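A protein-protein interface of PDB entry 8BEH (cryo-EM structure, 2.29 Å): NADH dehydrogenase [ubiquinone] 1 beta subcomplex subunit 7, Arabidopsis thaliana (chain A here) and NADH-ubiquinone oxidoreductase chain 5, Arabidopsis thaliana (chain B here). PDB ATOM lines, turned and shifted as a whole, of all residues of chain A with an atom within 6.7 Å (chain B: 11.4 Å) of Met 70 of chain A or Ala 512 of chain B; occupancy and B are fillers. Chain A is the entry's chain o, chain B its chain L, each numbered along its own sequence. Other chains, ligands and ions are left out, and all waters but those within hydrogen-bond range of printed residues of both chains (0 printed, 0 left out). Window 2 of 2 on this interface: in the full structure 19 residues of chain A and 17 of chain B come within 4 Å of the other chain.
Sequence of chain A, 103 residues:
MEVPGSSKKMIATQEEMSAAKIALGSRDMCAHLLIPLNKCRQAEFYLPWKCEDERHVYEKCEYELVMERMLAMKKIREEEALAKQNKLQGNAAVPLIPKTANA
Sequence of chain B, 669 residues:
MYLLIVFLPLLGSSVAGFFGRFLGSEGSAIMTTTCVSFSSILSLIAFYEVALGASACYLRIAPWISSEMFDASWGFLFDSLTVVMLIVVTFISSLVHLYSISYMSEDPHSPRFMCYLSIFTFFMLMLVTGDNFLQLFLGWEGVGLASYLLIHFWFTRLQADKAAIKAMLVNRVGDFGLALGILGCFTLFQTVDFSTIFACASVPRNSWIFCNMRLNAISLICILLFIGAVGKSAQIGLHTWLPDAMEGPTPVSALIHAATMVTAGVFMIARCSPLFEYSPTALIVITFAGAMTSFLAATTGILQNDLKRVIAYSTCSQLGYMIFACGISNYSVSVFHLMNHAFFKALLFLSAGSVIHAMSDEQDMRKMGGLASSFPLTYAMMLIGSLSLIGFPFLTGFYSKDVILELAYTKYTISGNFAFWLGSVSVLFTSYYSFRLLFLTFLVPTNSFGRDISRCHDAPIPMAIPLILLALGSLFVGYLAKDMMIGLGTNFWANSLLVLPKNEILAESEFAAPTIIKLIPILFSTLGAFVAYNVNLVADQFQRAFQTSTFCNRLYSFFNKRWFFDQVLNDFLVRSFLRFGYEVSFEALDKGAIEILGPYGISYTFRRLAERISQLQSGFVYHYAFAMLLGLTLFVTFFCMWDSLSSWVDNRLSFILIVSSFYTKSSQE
OE2 of Glu 508 of chain B lies within salt-bridge range of NH2 of Arg 69 of chain A (3.0 Å).
CA of Tyr 63 of chain A touches CD2 of Phe 511 of chain B, 3.7 Å away.
Ala 512 of chain B touches Val 66 of chain A.
Met 67 of chain A touches Phe 511 of chain B (CE to O, 3.6 Å).
CB of Ala 512 of chain B touches SD of Met 70 of chain A (3.7 Å).
Of chain B, only Ala 512 comes within 4 Å of Met 70 of chain A.
Ala 512 of chain B touches two residues of chain A.
Val 66 of chain A touches one residue of chain B.
Of the printed residues of chain B, Met 67 of chain A touches Phe 511 (3.6 Å).
Of chain B, only Glu 508 comes within 4 Å of Arg 69 of chain A.
No residue of chain B comes within 4 Å of Leu 71 of chain A.
No residue of chain B comes within 4 Å of Met 73 of chain A.
Of the printed residues of chain A, Glu 508 of chain B touches Arg 69.
Printed residues of chain A within 4 Å of Phe 511 of chain B: Tyr 63 and Met 67.
Lys 518 of chain B touches none of the printed residues of chain A.
Ser 509 of chain B touches none of the printed residues of chain A.
The nearest residue of chain A that does not touch Ala 512 of chain B is Met 67 of chain A (4.8 Å).
Of the 12 printed residues of chain A, 5 touch a printed residue of chain B.
Hydrophobic or aromatic side chains of chain A within 4 Å of the printed part of chain B: Tyr 63, Val 66, Met 67 and Met 70.
Of the 24 printed residues of chain B, 3 touch a printed residue of chain A.
Printed residues of chain B that touch a printed residue of chain A: Glu 508, Phe 511 and Ala 512.
Among the printed residues, 5 pairs touch across the chains.
Among the printed residues, Asp or Glu carboxylates within 4 Å of a Lys or Arg side-chain nitrogen of the other chain: Arg 69 of chain A with Glu 508 of chain B (3.0 Å).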
ATOM      1  N   TYR A  63     -33.540 -10.143  22.458  1.00  0.00           N
ATOM      2  CA  TYR A  63     -33.303 -11.575  22.349  1.00  0.00           C
ATOM      3  C   TYR A  63     -34.534 -12.292  21.812  1.00  0.00           C
ATOM      4  O   TYR A  63     -34.414 -13.183  20.967  1.00  0.00           O
ATOM      5  CB  TYR A  63     -32.885 -12.136  23.709  1.00  0.00           C
ATOM      6  CG  TYR A  63     -32.934 -13.644  23.825  1.00  0.00           C
ATOM      7  CD1 TYR A  63     -34.096 -14.293  24.224  1.00  0.00           C
ATOM      8  CD2 TYR A  63     -31.816 -14.421  23.547  1.00  0.00           C
ATOM      9  CE1 TYR A  63     -34.148 -15.659  24.334  1.00  0.00           C
ATOM     10  CE2 TYR A  63     -31.858 -15.795  23.658  1.00  0.00           C
ATOM     11  CZ  TYR A  63     -33.029 -16.407  24.047  1.00  0.00           C
ATOM     12  OH  TYR A  63     -33.088 -17.774  24.157  1.00  0.00           O
ATOM     13  N   LEU A  65     -36.843 -11.018  19.861  1.00  0.00           N
ATOM     14  CA  LEU A  65     -36.927 -10.704  18.433  1.00  0.00           C
ATOM     15  C   LEU A  65     -36.033 -11.634  17.613  1.00  0.00           C
ATOM     16  O   LEU A  65     -36.467 -12.228  16.608  1.00  0.00           O
ATOM     17  CB  LEU A  65     -36.538  -9.243  18.194  1.00  0.00           C
ATOM     18  CG  LEU A  65     -37.613  -8.157  18.264  1.00  0.00           C
ATOM     19  CD1 LEU A  65     -37.185  -6.921  17.485  1.00  0.00           C
ATOM     20  CD2 LEU A  65     -38.949  -8.668  17.754  1.00  0.00           C
ATOM     21  N   VAL A  66     -34.780 -11.783  18.047  1.00  0.00           N
ATOM     22  CA  VAL A  66     -33.850 -12.655  17.334  1.00  0.00           C
ATOM     23  C   VAL A  66     -34.341 -14.097  17.346  1.00  0.00           C
ATOM     24  O   VAL A  66     -34.224 -14.813  16.347  1.00  0.00           O
ATOM     25  CB  VAL A  66     -32.432 -12.535  17.920  1.00  0.00           C
ATOM     26  CG1 VAL A  66     -31.463 -13.365  17.111  1.00  0.00           C
ATOM     27  CG2 VAL A  66     -31.988 -11.092  17.918  1.00  0.00           C
ATOM     28  N   MET A  67     -34.886 -14.548  18.474  1.00  0.00           N
ATOM     29  CA  MET A  67     -35.367 -15.925  18.557  1.00  0.00           C
ATOM     30  C   MET A  67     -36.520 -16.171  17.592  1.00  0.00           C
ATOM     31  O   MET A  67     -36.587 -17.228  16.959  1.00  0.00           O
ATOM     32  CB  MET A  67     -35.778 -16.259  19.987  1.00  0.00           C
ATOM     33  CG  MET A  67     -34.609 -16.428  20.924  1.00  0.00           C
ATOM     34  SD  MET A  67     -33.335 -17.491  20.230  1.00  0.00           S
ATOM     35  CE  MET A  67     -31.946 -16.362  20.199  1.00  0.00           C
ATOM     36  N   GLU A  68     -37.440 -15.212  17.470  1.00  0.00           N
ATOM     37  CA  GLU A  68     -38.533 -15.383  16.516  1.00  0.00           C
ATOM     38  C   GLU A  68     -38.003 -15.475  15.093  1.00  0.00           C
ATOM     39  O   GLU A  68     -38.470 -16.299  14.299  1.00  0.00           O
ATOM     40  CB  GLU A  68     -39.548 -14.246  16.632  1.00  0.00           C
ATOM     41  CG  GLU A  68     -40.070 -14.012  18.028  1.00  0.00           C
ATOM     42  CD  GLU A  68     -40.801 -12.692  18.158  1.00  0.00           C
ATOM     43  OE1 GLU A  68     -40.150 -11.634  18.034  1.00  0.00           O
ATOM     44  OE2 GLU A  68     -42.031 -12.713  18.383  1.00  0.00           O
ATOM     45  N   ARG A  69     -37.061 -14.663  14.679  1.00  0.00           N
ATOM     46  CA  ARG A  69     -36.422 -14.742  13.342  1.00  0.00           C
ATOM     47  C   ARG A  69     -35.606 -16.044  13.192  1.00  0.00           C
ATOM     48  O   ARG A  69     -35.463 -16.521  12.097  1.00  0.00           O
ATOM     49  CB  ARG A  69     -35.707 -13.394  13.134  1.00  0.00           C
ATOM     50  CG  ARG A  69     -36.545 -12.190  12.760  1.00  0.00           C
ATOM     51  CD  ARG A  69     -35.676 -10.944  12.808  1.00  0.00           C
ATOM     52  NE  ARG A  69     -34.414 -11.117  12.108  1.00  0.00           N
ATOM     53  CZ  ARG A  69     -33.238 -10.682  12.531  1.00  0.00           C
ATOM     54  NH1 ARG A  69     -33.142 -10.002  13.655  1.00  0.00           N
ATOM     55  NH2 ARG A  69     -32.157 -10.914  11.814  1.00  0.00           N
ATOM     56  N   MET A  70     -35.104 -16.613  14.271  1.00  0.00           N
ATOM     57  CA  MET A  70     -34.451 -17.917  14.177  1.00  0.00           C
ATOM     58  C   MET A  70     -35.462 -19.040  13.950  1.00  0.00           C
ATOM     59  O   MET A  70     -35.228 -19.936  13.133  1.00  0.00           O
ATOM     60  CB  MET A  70     -33.623 -18.181  15.433  1.00  0.00           C
ATOM     61  CG  MET A  70     -32.427 -17.264  15.593  1.00  0.00           C
ATOM     62  SD  MET A  70     -31.316 -17.734  16.929  1.00  0.00           S
ATOM     63  CE  MET A  70     -30.488 -19.145  16.211  1.00  0.00           C
ATOM     64  N   LEU A  71     -36.591 -19.015  14.670  1.00  0.00           N
ATOM     65  CA  LEU A  71     -37.626 -20.025  14.437  1.00  0.00           C
ATOM     66  C   LEU A  71     -38.226 -19.898  13.043  1.00  0.00           C
ATOM     67  O   LEU A  71     -38.524 -20.910  12.394  1.00  0.00           O
ATOM     68  CB  LEU A  71     -38.728 -19.950  15.497  1.00  0.00           C
ATOM     69  CG  LEU A  71     -38.485 -20.689  16.818  1.00  0.00           C
ATOM     70  CD1 LEU A  71     -38.011 -19.768  17.927  1.00  0.00           C
ATOM     71  CD2 LEU A  71     -39.738 -21.431  17.238  1.00  0.00           C
ATOM     72  N   ALA A  72     -38.415 -18.669  12.564  1.00  0.00           N
ATOM     73  CA  ALA A  72     -38.909 -18.478  11.205  1.00  0.00           C
ATOM     74  C   ALA A  72     -37.961 -19.100  10.185  1.00  0.00           C
ATOM     75  O   ALA A  72     -38.395 -19.799   9.258  1.00  0.00           O
ATOM     76  CB  ALA A  72     -39.102 -16.990  10.927  1.00  0.00           C
ATOM     77  N   MET A  73     -36.654 -18.868  10.346  1.00  0.00           N
ATOM     78  CA  MET A  73     -35.703 -19.477   9.420  1.00  0.00           C
ATOM     79  C   MET A  73     -35.667 -20.993   9.571  1.00  0.00           C
ATOM     80  O   MET A  73     -35.443 -21.702   8.588  1.00  0.00           O
ATOM     81  CB  MET A  73     -34.307 -18.888   9.619  1.00  0.00           C
ATOM     82  CG  MET A  73     -33.253 -19.430   8.663  1.00  0.00           C
ATOM     83  SD  MET A  73     -33.731 -19.363   6.923  1.00  0.00           S
ATOM     84  CE  MET A  73     -33.434 -17.644   6.531  1.00  0.00           C
ATOM     85  N   LYS A  74     -35.873 -21.507  10.784  1.00  0.00           N
ATOM     86  CA  LYS A  74     -35.967 -22.951  10.972  1.00  0.00           C
ATOM     87  C   LYS A  74     -37.121 -23.530  10.159  1.00  0.00           C
ATOM     88  O   LYS A  74     -36.968 -24.548   9.477  1.00  0.00           O
ATOM     89  CB  LYS A  74     -36.143 -23.273  12.456  1.00  0.00           C
ATOM     90  CG  LYS A  74     -36.181 -24.747  12.780  1.00  0.00           C
ATOM     91  CD  LYS A  74     -36.308 -24.973  14.278  1.00  0.00           C
ATOM     92  CE  LYS A  74     -36.373 -26.451  14.625  1.00  0.00           C
ATOM     93  NZ  LYS A  74     -36.497 -26.658  16.093  1.00  0.00           N
ATOM     94  N   LYS A  75     -38.325 -22.921  10.183  1.00  0.00           N
ATOM     95  CA  LYS A  75     -39.470 -23.320   9.293  1.00  0.00           C
ATOM     96  C   LYS A  75     -39.181 -23.280   7.780  1.00  0.00           C
ATOM     97  O   LYS A  75     -39.373 -24.304   7.167  1.00  0.00           O
ATOM     98  CB  LYS A  75     -40.783 -22.594   9.623  1.00  0.00           C
ATOM     99  CG  LYS A  75     -41.676 -23.284  10.635  1.00  0.00           C
ATOM    100  CD  LYS A  75     -43.044 -22.649  10.785  1.00  0.00           C
ATOM    101  CE  LYS A  75     -43.794 -22.536   9.475  1.00  0.00           C
ATOM    102  NZ  LYS A  75     -43.881 -23.839   8.774  1.00  0.00           N
ATOM    103  N   LEU B 405     -14.688 -10.377  16.607  1.00  0.00           N
ATOM    104  CA  LEU B 405     -14.663 -11.723  16.039  1.00  0.00           C
ATOM    105  C   LEU B 405     -16.071 -12.316  15.937  1.00  0.00           C
ATOM    106  O   LEU B 405     -16.414 -12.950  14.931  1.00  0.00           O
ATOM    107  CB  LEU B 405     -13.740 -12.617  16.864  1.00  0.00           C
ATOM    108  CG  LEU B 405     -12.265 -12.600  16.441  1.00  0.00           C
ATOM    109  CD1 LEU B 405     -11.475 -13.662  17.177  1.00  0.00           C
ATOM    110  CD2 LEU B 405     -12.100 -12.758  14.933  1.00  0.00           C
ATOM    111  N   GLU B 406     -16.908 -12.133  16.934  1.00  0.00           N
ATOM    112  CA  GLU B 406     -18.312 -12.571  16.931  1.00  0.00           C
ATOM    113  C   GLU B 406     -19.121 -11.889  15.844  1.00  0.00           C
ATOM    114  O   GLU B 406     -19.892 -12.597  15.235  1.00  0.00           O
ATOM    115  CB  GLU B 406     -18.924 -12.188  18.290  1.00  0.00           C
ATOM    116  CG  GLU B 406     -18.738 -13.224  19.360  1.00  0.00           C
ATOM    117  CD  GLU B 406     -18.773 -12.581  20.726  1.00  0.00           C
ATOM    118  OE1 GLU B 406     -19.729 -11.841  21.000  1.00  0.00           O
ATOM    119  OE2 GLU B 406     -17.831 -12.790  21.491  1.00  0.00           O
ATOM    120  N   LEU B 407     -18.895 -10.568  15.622  1.00  0.00           N
ATOM    121  CA  LEU B 407     -19.569  -9.853  14.546  1.00  0.00           C
ATOM    122  C   LEU B 407     -19.137 -10.378  13.187  1.00  0.00           C
ATOM    123  O   LEU B 407     -19.962 -10.521  12.277  1.00  0.00           O
ATOM    124  CB  LEU B 407     -19.289  -8.354  14.652  1.00  0.00           C
ATOM    125  CG  LEU B 407     -19.962  -7.568  15.776  1.00  0.00           C
ATOM    126  CD1 LEU B 407     -19.298  -6.215  15.952  1.00  0.00           C
ATOM    127  CD2 LEU B 407     -21.447  -7.409  15.499  1.00  0.00           C
ATOM    128  N   ALA B 408     -17.874 -10.750  13.042  1.00  0.00           N
ATOM    129  CA  ALA B 408     -17.407 -11.287  11.755  1.00  0.00           C
ATOM    130  C   ALA B 408     -18.076 -12.625  11.514  1.00  0.00           C
ATOM    131  O   ALA B 408     -18.417 -12.920  10.420  1.00  0.00           O
ATOM    132  CB  ALA B 408     -15.929 -11.433  11.750  1.00  0.00           C
ATOM    133  N   TYR B 409     -18.157 -13.400  12.588  1.00  0.00           N
ATOM    134  CA  TYR B 409     -18.864 -14.666  12.445  1.00  0.00           C
ATOM    135  C   TYR B 409     -20.302 -14.443  11.989  1.00  0.00           C
ATOM    136  O   TYR B 409     -20.840 -15.223  11.196  1.00  0.00           O
ATOM    137  CB  TYR B 409     -18.843 -15.436  13.761  1.00  0.00           C
ATOM    138  CG  TYR B 409     -19.687 -16.680  13.715  1.00  0.00           C
ATOM    139  CD1 TYR B 409     -19.224 -17.827  13.090  1.00  0.00           C
ATOM    140  CD2 TYR B 409     -20.965 -16.699  14.261  1.00  0.00           C
ATOM    141  CE1 TYR B 409     -19.995 -18.964  13.031  1.00  0.00           C
ATOM    142  CE2 TYR B 409     -21.743 -17.833  14.205  1.00  0.00           C
ATOM    143  CZ  TYR B 409     -21.254 -18.961  13.589  1.00  0.00           C
ATOM    144  OH  TYR B 409     -22.025 -20.093  13.531  1.00  0.00           O
ATOM    145  N   THR B 410     -20.938 -13.387  12.487  1.00  0.00           N
ATOM    146  CA  THR B 410     -22.337 -13.120  12.180  1.00  0.00           C
ATOM    147  C   THR B 410     -22.542 -12.503  10.797  1.00  0.00           C
ATOM    148  O   THR B 410     -23.668 -12.506  10.292  1.00  0.00           O
ATOM    149  CB  THR B 410     -22.919 -12.223  13.275  1.00  0.00           C
ATOM    150  OG1 THR B 410     -22.520 -12.739  14.548  1.00  0.00           O
ATOM    151  CG2 THR B 410     -24.431 -12.185  13.221  1.00  0.00           C
ATOM    152  N   LYS B 411     -21.490 -11.999  10.159  1.00  0.00           N
ATOM    153  CA  LYS B 411     -21.618 -11.455   8.808  1.00  0.00           C
ATOM    154  C   LYS B 411     -21.663 -12.611   7.817  1.00  0.00           C
ATOM    155  O   LYS B 411     -20.634 -13.200   7.478  1.00  0.00           O
ATOM    156  CB  LYS B 411     -20.475 -10.496   8.502  1.00  0.00           C
ATOM    157  CG  LYS B 411     -20.651  -9.716   7.219  1.00  0.00           C
ATOM    158  CD  LYS B 411     -21.167  -8.315   7.483  1.00  0.00           C
ATOM    159  CE  LYS B 411     -21.455  -7.575   6.189  1.00  0.00           C
ATOM    160  NZ  LYS B 411     -22.755  -6.862   6.217  1.00  0.00           N
ATOM    161  N   TYR B 412     -22.863 -12.940   7.340  1.00  0.00           N
ATOM    162  CA  TYR B 412     -23.051 -14.088   6.453  1.00  0.00           C
ATOM    163  C   TYR B 412     -22.824 -13.662   5.002  1.00  0.00           C
ATOM    164  O   TYR B 412     -23.731 -13.605   4.174  1.00  0.00           O
ATOM    165  CB  TYR B 412     -24.426 -14.707   6.668  1.00  0.00           C
ATOM    166  CG  TYR B 412     -24.445 -15.690   7.813  1.00  0.00           C
ATOM    167  CD1 TYR B 412     -24.606 -15.259   9.120  1.00  0.00           C
ATOM    168  CD2 TYR B 412     -24.269 -17.045   7.590  1.00  0.00           C
ATOM    169  CE1 TYR B 412     -24.609 -16.150  10.169  1.00  0.00           C
ATOM    170  CE2 TYR B 412     -24.265 -17.943   8.629  1.00  0.00           C
ATOM    171  CZ  TYR B 412     -24.435 -17.491   9.918  1.00  0.00           C
ATOM    172  OH  TYR B 412     -24.434 -18.385  10.959  1.00  0.00           O
ATOM    173  N   LEU B 488     -26.019  -2.244  23.576  1.00  0.00           N
ATOM    174  CA  LEU B 488     -27.156  -2.410  22.679  1.00  0.00           C
ATOM    175  C   LEU B 488     -28.073  -1.194  22.703  1.00  0.00           C
ATOM    176  O   LEU B 488     -28.630  -0.842  23.745  1.00  0.00           O
ATOM    177  CB  LEU B 488     -27.937  -3.667  23.065  1.00  0.00           C
ATOM    178  CG  LEU B 488     -28.411  -4.563  21.923  1.00  0.00           C
ATOM    179  CD1 LEU B 488     -27.233  -5.059  21.110  1.00  0.00           C
ATOM    180  CD2 LEU B 488     -29.239  -5.728  22.444  1.00  0.00           C
ATOM    181  N   GLU B 504     -27.269  -3.788  10.439  1.00  0.00           N
ATOM    182  CA  GLU B 504     -27.232  -3.960  11.915  1.00  0.00           C
ATOM    183  C   GLU B 504     -27.181  -5.461  12.282  1.00  0.00           C
ATOM    184  O   GLU B 504     -28.085  -6.185  11.950  1.00  0.00           O
ATOM    185  CB  GLU B 504     -28.335  -3.113  12.586  1.00  0.00           C
ATOM    186  CG  GLU B 504     -27.957  -1.688  12.921  1.00  0.00           C
ATOM    187  CD  GLU B 504     -26.808  -1.398  13.881  1.00  0.00           C
ATOM    188  OE1 GLU B 504     -26.068  -2.321  14.259  1.00  0.00           O
ATOM    189  OE2 GLU B 504     -26.653  -0.226  14.247  1.00  0.00           O
ATOM    190  N   ILE B 505     -26.132  -5.891  12.931  1.00  0.00           N
ATOM    191  CA  ILE B 505     -25.894  -7.308  13.317  1.00  0.00           C
ATOM    192  C   ILE B 505     -25.507  -7.467  14.790  1.00  0.00           C
ATOM    193  O   ILE B 505     -25.266  -8.591  15.156  1.00  0.00           O
ATOM    194  CB  ILE B 505     -24.783  -7.944  12.428  1.00  0.00           C
ATOM    195  CG1 ILE B 505     -23.445  -7.213  12.548  1.00  0.00           C
ATOM    196  CG2 ILE B 505     -25.210  -8.085  10.971  1.00  0.00           C
ATOM    197  CD1 ILE B 505     -22.315  -7.910  11.836  1.00  0.00           C
ATOM    198  N   LEU B 506     -25.440  -6.434  15.591  1.00  0.00           N
ATOM    199  CA  LEU B 506     -24.946  -6.580  16.981  1.00  0.00           C
ATOM    200  C   LEU B 506     -25.841  -7.538  17.843  1.00  0.00           C
ATOM    201  O   LEU B 506     -25.253  -8.404  18.476  1.00  0.00           O
ATOM    202  CB  LEU B 506     -24.769  -5.229  17.626  1.00  0.00           C
ATOM    203  CG  LEU B 506     -24.110  -5.235  19.004  1.00  0.00           C
ATOM    204  CD1 LEU B 506     -22.660  -5.695  18.945  1.00  0.00           C
ATOM    205  CD2 LEU B 506     -24.220  -3.875  19.666  1.00  0.00           C
ATOM    206  N   ALA B 507     -27.161  -7.424  17.820  1.00  0.00           N
ATOM    207  CA  ALA B 507     -28.106  -8.326  18.556  1.00  0.00           C
ATOM    208  C   ALA B 507     -27.872  -9.781  18.177  1.00  0.00           C
ATOM    209  O   ALA B 507     -27.576 -10.530  19.065  1.00  0.00           O
ATOM    210  CB  ALA B 507     -29.530  -7.911  18.303  1.00  0.00           C
ATOM    211  N   GLU B 508     -27.897 -10.096  16.890  1.00  0.00           N
ATOM    212  CA  GLU B 508     -27.702 -11.462  16.375  1.00  0.00           C
ATOM    213  C   GLU B 508     -26.322 -12.005  16.792  1.00  0.00           C
ATOM    214  O   GLU B 508     -26.239 -13.198  16.972  1.00  0.00           O
ATOM    215  CB  GLU B 508     -27.988 -11.518  14.859  1.00  0.00           C
ATOM    216  CG  GLU B 508     -29.312 -10.950  14.422  1.00  0.00           C
ATOM    217  CD  GLU B 508     -29.271  -9.522  13.908  1.00  0.00           C
ATOM    218  OE1 GLU B 508     -28.700  -8.665  14.582  1.00  0.00           O
ATOM    219  OE2 GLU B 508     -29.816  -9.280  12.842  1.00  0.00           O
ATOM    220  N   SER B 509     -25.298 -11.174  16.889  1.00  0.00           N
ATOM    221  CA  SER B 509     -23.976 -11.626  17.387  1.00  0.00           C
ATOM    222  C   SER B 509     -24.015 -11.890  18.912  1.00  0.00           C
ATOM    223  O   SER B 509     -23.336 -12.772  19.361  1.00  0.00           O
ATOM    224  CB  SER B 509     -22.874 -10.675  17.015  1.00  0.00           C
ATOM    225  OG  SER B 509     -22.673  -9.648  17.965  1.00  0.00           O
ATOM    226  N   GLU B 510     -24.726 -11.093  19.656  1.00  0.00           N
ATOM    227  CA  GLU B 510     -24.821 -11.395  21.081  1.00  0.00           C
ATOM    228  C   GLU B 510     -25.846 -12.494  21.398  1.00  0.00           C
ATOM    229  O   GLU B 510     -25.766 -13.014  22.474  1.00  0.00           O
ATOM    230  CB  GLU B 510     -25.057 -10.122  21.881  1.00  0.00           C
ATOM    231  CG  GLU B 510     -26.417  -9.512  21.894  1.00  0.00           C
ATOM    232  CD  GLU B 510     -26.489  -8.694  23.168  1.00  0.00           C
ATOM    233  OE1 GLU B 510     -25.939  -9.137  24.190  1.00  0.00           O
ATOM    234  OE2 GLU B 510     -27.077  -7.618  23.139  1.00  0.00           O
ATOM    235  N   PHE B 511     -26.671 -12.905  20.453  1.00  0.00           N
ATOM    236  CA  PHE B 511     -27.779 -13.757  20.876  1.00  0.00           C
ATOM    237  C   PHE B 511     -27.930 -15.026  20.040  1.00  0.00           C
ATOM    238  O   PHE B 511     -28.335 -16.066  20.564  1.00  0.00           O
ATOM    239  CB  PHE B 511     -29.086 -12.960  20.855  1.00  0.00           C
ATOM    240  CG  PHE B 511     -29.186 -11.937  21.949  1.00  0.00           C
ATOM    241  CD1 PHE B 511     -28.719 -12.214  23.220  1.00  0.00           C
ATOM    242  CD2 PHE B 511     -29.732 -10.687  21.701  1.00  0.00           C
ATOM    243  CE1 PHE B 511     -28.799 -11.270  24.224  1.00  0.00           C
ATOM    244  CE2 PHE B 511     -29.817  -9.741  22.702  1.00  0.00           C
ATOM    245  CZ  PHE B 511     -29.349 -10.032  23.964  1.00  0.00           C
ATOM    246  N   ALA B 512     -27.627 -14.960  18.746  1.00  0.00           N
ATOM    247  CA  ALA B 512     -27.826 -16.086  17.844  1.00  0.00           C
ATOM    248  C   ALA B 512     -26.558 -16.898  17.609  1.00  0.00           C
ATOM    249  O   ALA B 512     -26.564 -17.810  16.778  1.00  0.00           O
ATOM    250  CB  ALA B 512     -28.383 -15.601  16.504  1.00  0.00           C
ATOM    251  N   ALA B 513     -25.475 -16.617  18.328  1.00  0.00           N
ATOM    252  CA  ALA B 513     -24.221 -17.344  18.044  1.00  0.00           C
ATOM    253  C   ALA B 513     -24.117 -18.562  18.952  1.00  0.00           C
ATOM    254  O   ALA B 513     -24.343 -18.443  20.139  1.00  0.00           O
ATOM    255  CB  ALA B 513     -23.012 -16.494  18.213  1.00  0.00           C
ATOM    256  N   PRO B 514     -23.631 -19.684  18.434  1.00  0.00           N
ATOM    257  CA  PRO B 514     -23.406 -20.836  19.273  1.00  0.00           C
ATOM    258  C   PRO B 514     -22.413 -20.414  20.353  1.00  0.00           C
ATOM    259  O   PRO B 514     -21.466 -19.695  20.042  1.00  0.00           O
ATOM    260  CB  PRO B 514     -22.816 -21.806  18.256  1.00  0.00           C
ATOM    261  CG  PRO B 514     -23.228 -21.336  16.900  1.00  0.00           C
ATOM    262  CD  PRO B 514     -23.255 -19.839  17.029  1.00  0.00           C
ATOM    263  N   THR B 515     -22.623 -20.825  21.592  1.00  0.00           N
ATOM    264  CA  THR B 515     -21.688 -20.546  22.706  1.00  0.00           C
ATOM    265  C   THR B 515     -20.221 -20.883  22.372  1.00  0.00           C
ATOM    266  O   THR B 515     -19.367 -20.196  22.889  1.00  0.00           O
ATOM    267  CB  THR B 515     -22.056 -21.358  23.966  1.00  0.00           C
ATOM    268  OG1 THR B 515     -22.232 -22.715  23.564  1.00  0.00           O
ATOM    269  CG2 THR B 515     -23.281 -20.831  24.677  1.00  0.00           C
ATOM    270  N   ILE B 516     -19.948 -21.923  21.577  1.00  0.00           N
ATOM    271  CA  ILE B 516     -18.551 -22.266  21.208  1.00  0.00           C
ATOM    272  C   ILE B 516     -17.862 -21.058  20.572  1.00  0.00           C
ATOM    273  O   ILE B 516     -16.732 -20.813  20.972  1.00  0.00           O
ATOM    274  CB  ILE B 516     -18.451 -23.491  20.250  1.00  0.00           C
ATOM    275  CG1 ILE B 516     -17.035 -24.065  20.216  1.00  0.00           C
ATOM    276  CG2 ILE B 516     -18.977 -23.237  18.852  1.00  0.00           C
ATOM    277  CD1 ILE B 516     -16.446 -24.316  21.572  1.00  0.00           C
ATOM    278  N   ILE B 517     -18.509 -20.399  19.615  1.00  0.00           N
ATOM    279  CA  ILE B 517     -17.929 -19.301  18.820  1.00  0.00           C
ATOM    280  C   ILE B 517     -17.312 -18.292  19.756  1.00  0.00           C
ATOM    281  O   ILE B 517     -16.251 -17.807  19.459  1.00  0.00           O
ATOM    282  CB  ILE B 517     -18.971 -18.744  17.807  1.00  0.00           C
ATOM    283  CG1 ILE B 517     -19.308 -19.737  16.693  1.00  0.00           C
ATOM    284  CG2 ILE B 517     -18.523 -17.408  17.226  1.00  0.00           C
ATOM    285  CD1 ILE B 517     -18.123 -20.244  15.922  1.00  0.00           C
ATOM    286  N   LYS B 518     -17.922 -18.111  20.913  1.00  0.00           N
ATOM    287  CA  LYS B 518     -17.456 -17.082  21.847  1.00  0.00           C
ATOM    288  C   LYS B 518     -16.191 -17.537  22.577  1.00  0.00           C
ATOM    289  O   LYS B 518     -15.539 -16.697  23.110  1.00  0.00           O
ATOM    290  CB  LYS B 518     -18.668 -16.729  22.710  1.00  0.00           C
ATOM    291  CG  LYS B 518     -19.972 -16.661  21.923  1.00  0.00           C
ATOM    292  CD  LYS B 518     -21.213 -16.572  22.788  1.00  0.00           C
ATOM    293  CE  LYS B 518     -21.814 -15.184  22.834  1.00  0.00           C
ATOM    294  NZ  LYS B 518     -22.382 -14.780  21.527  1.00  0.00           N
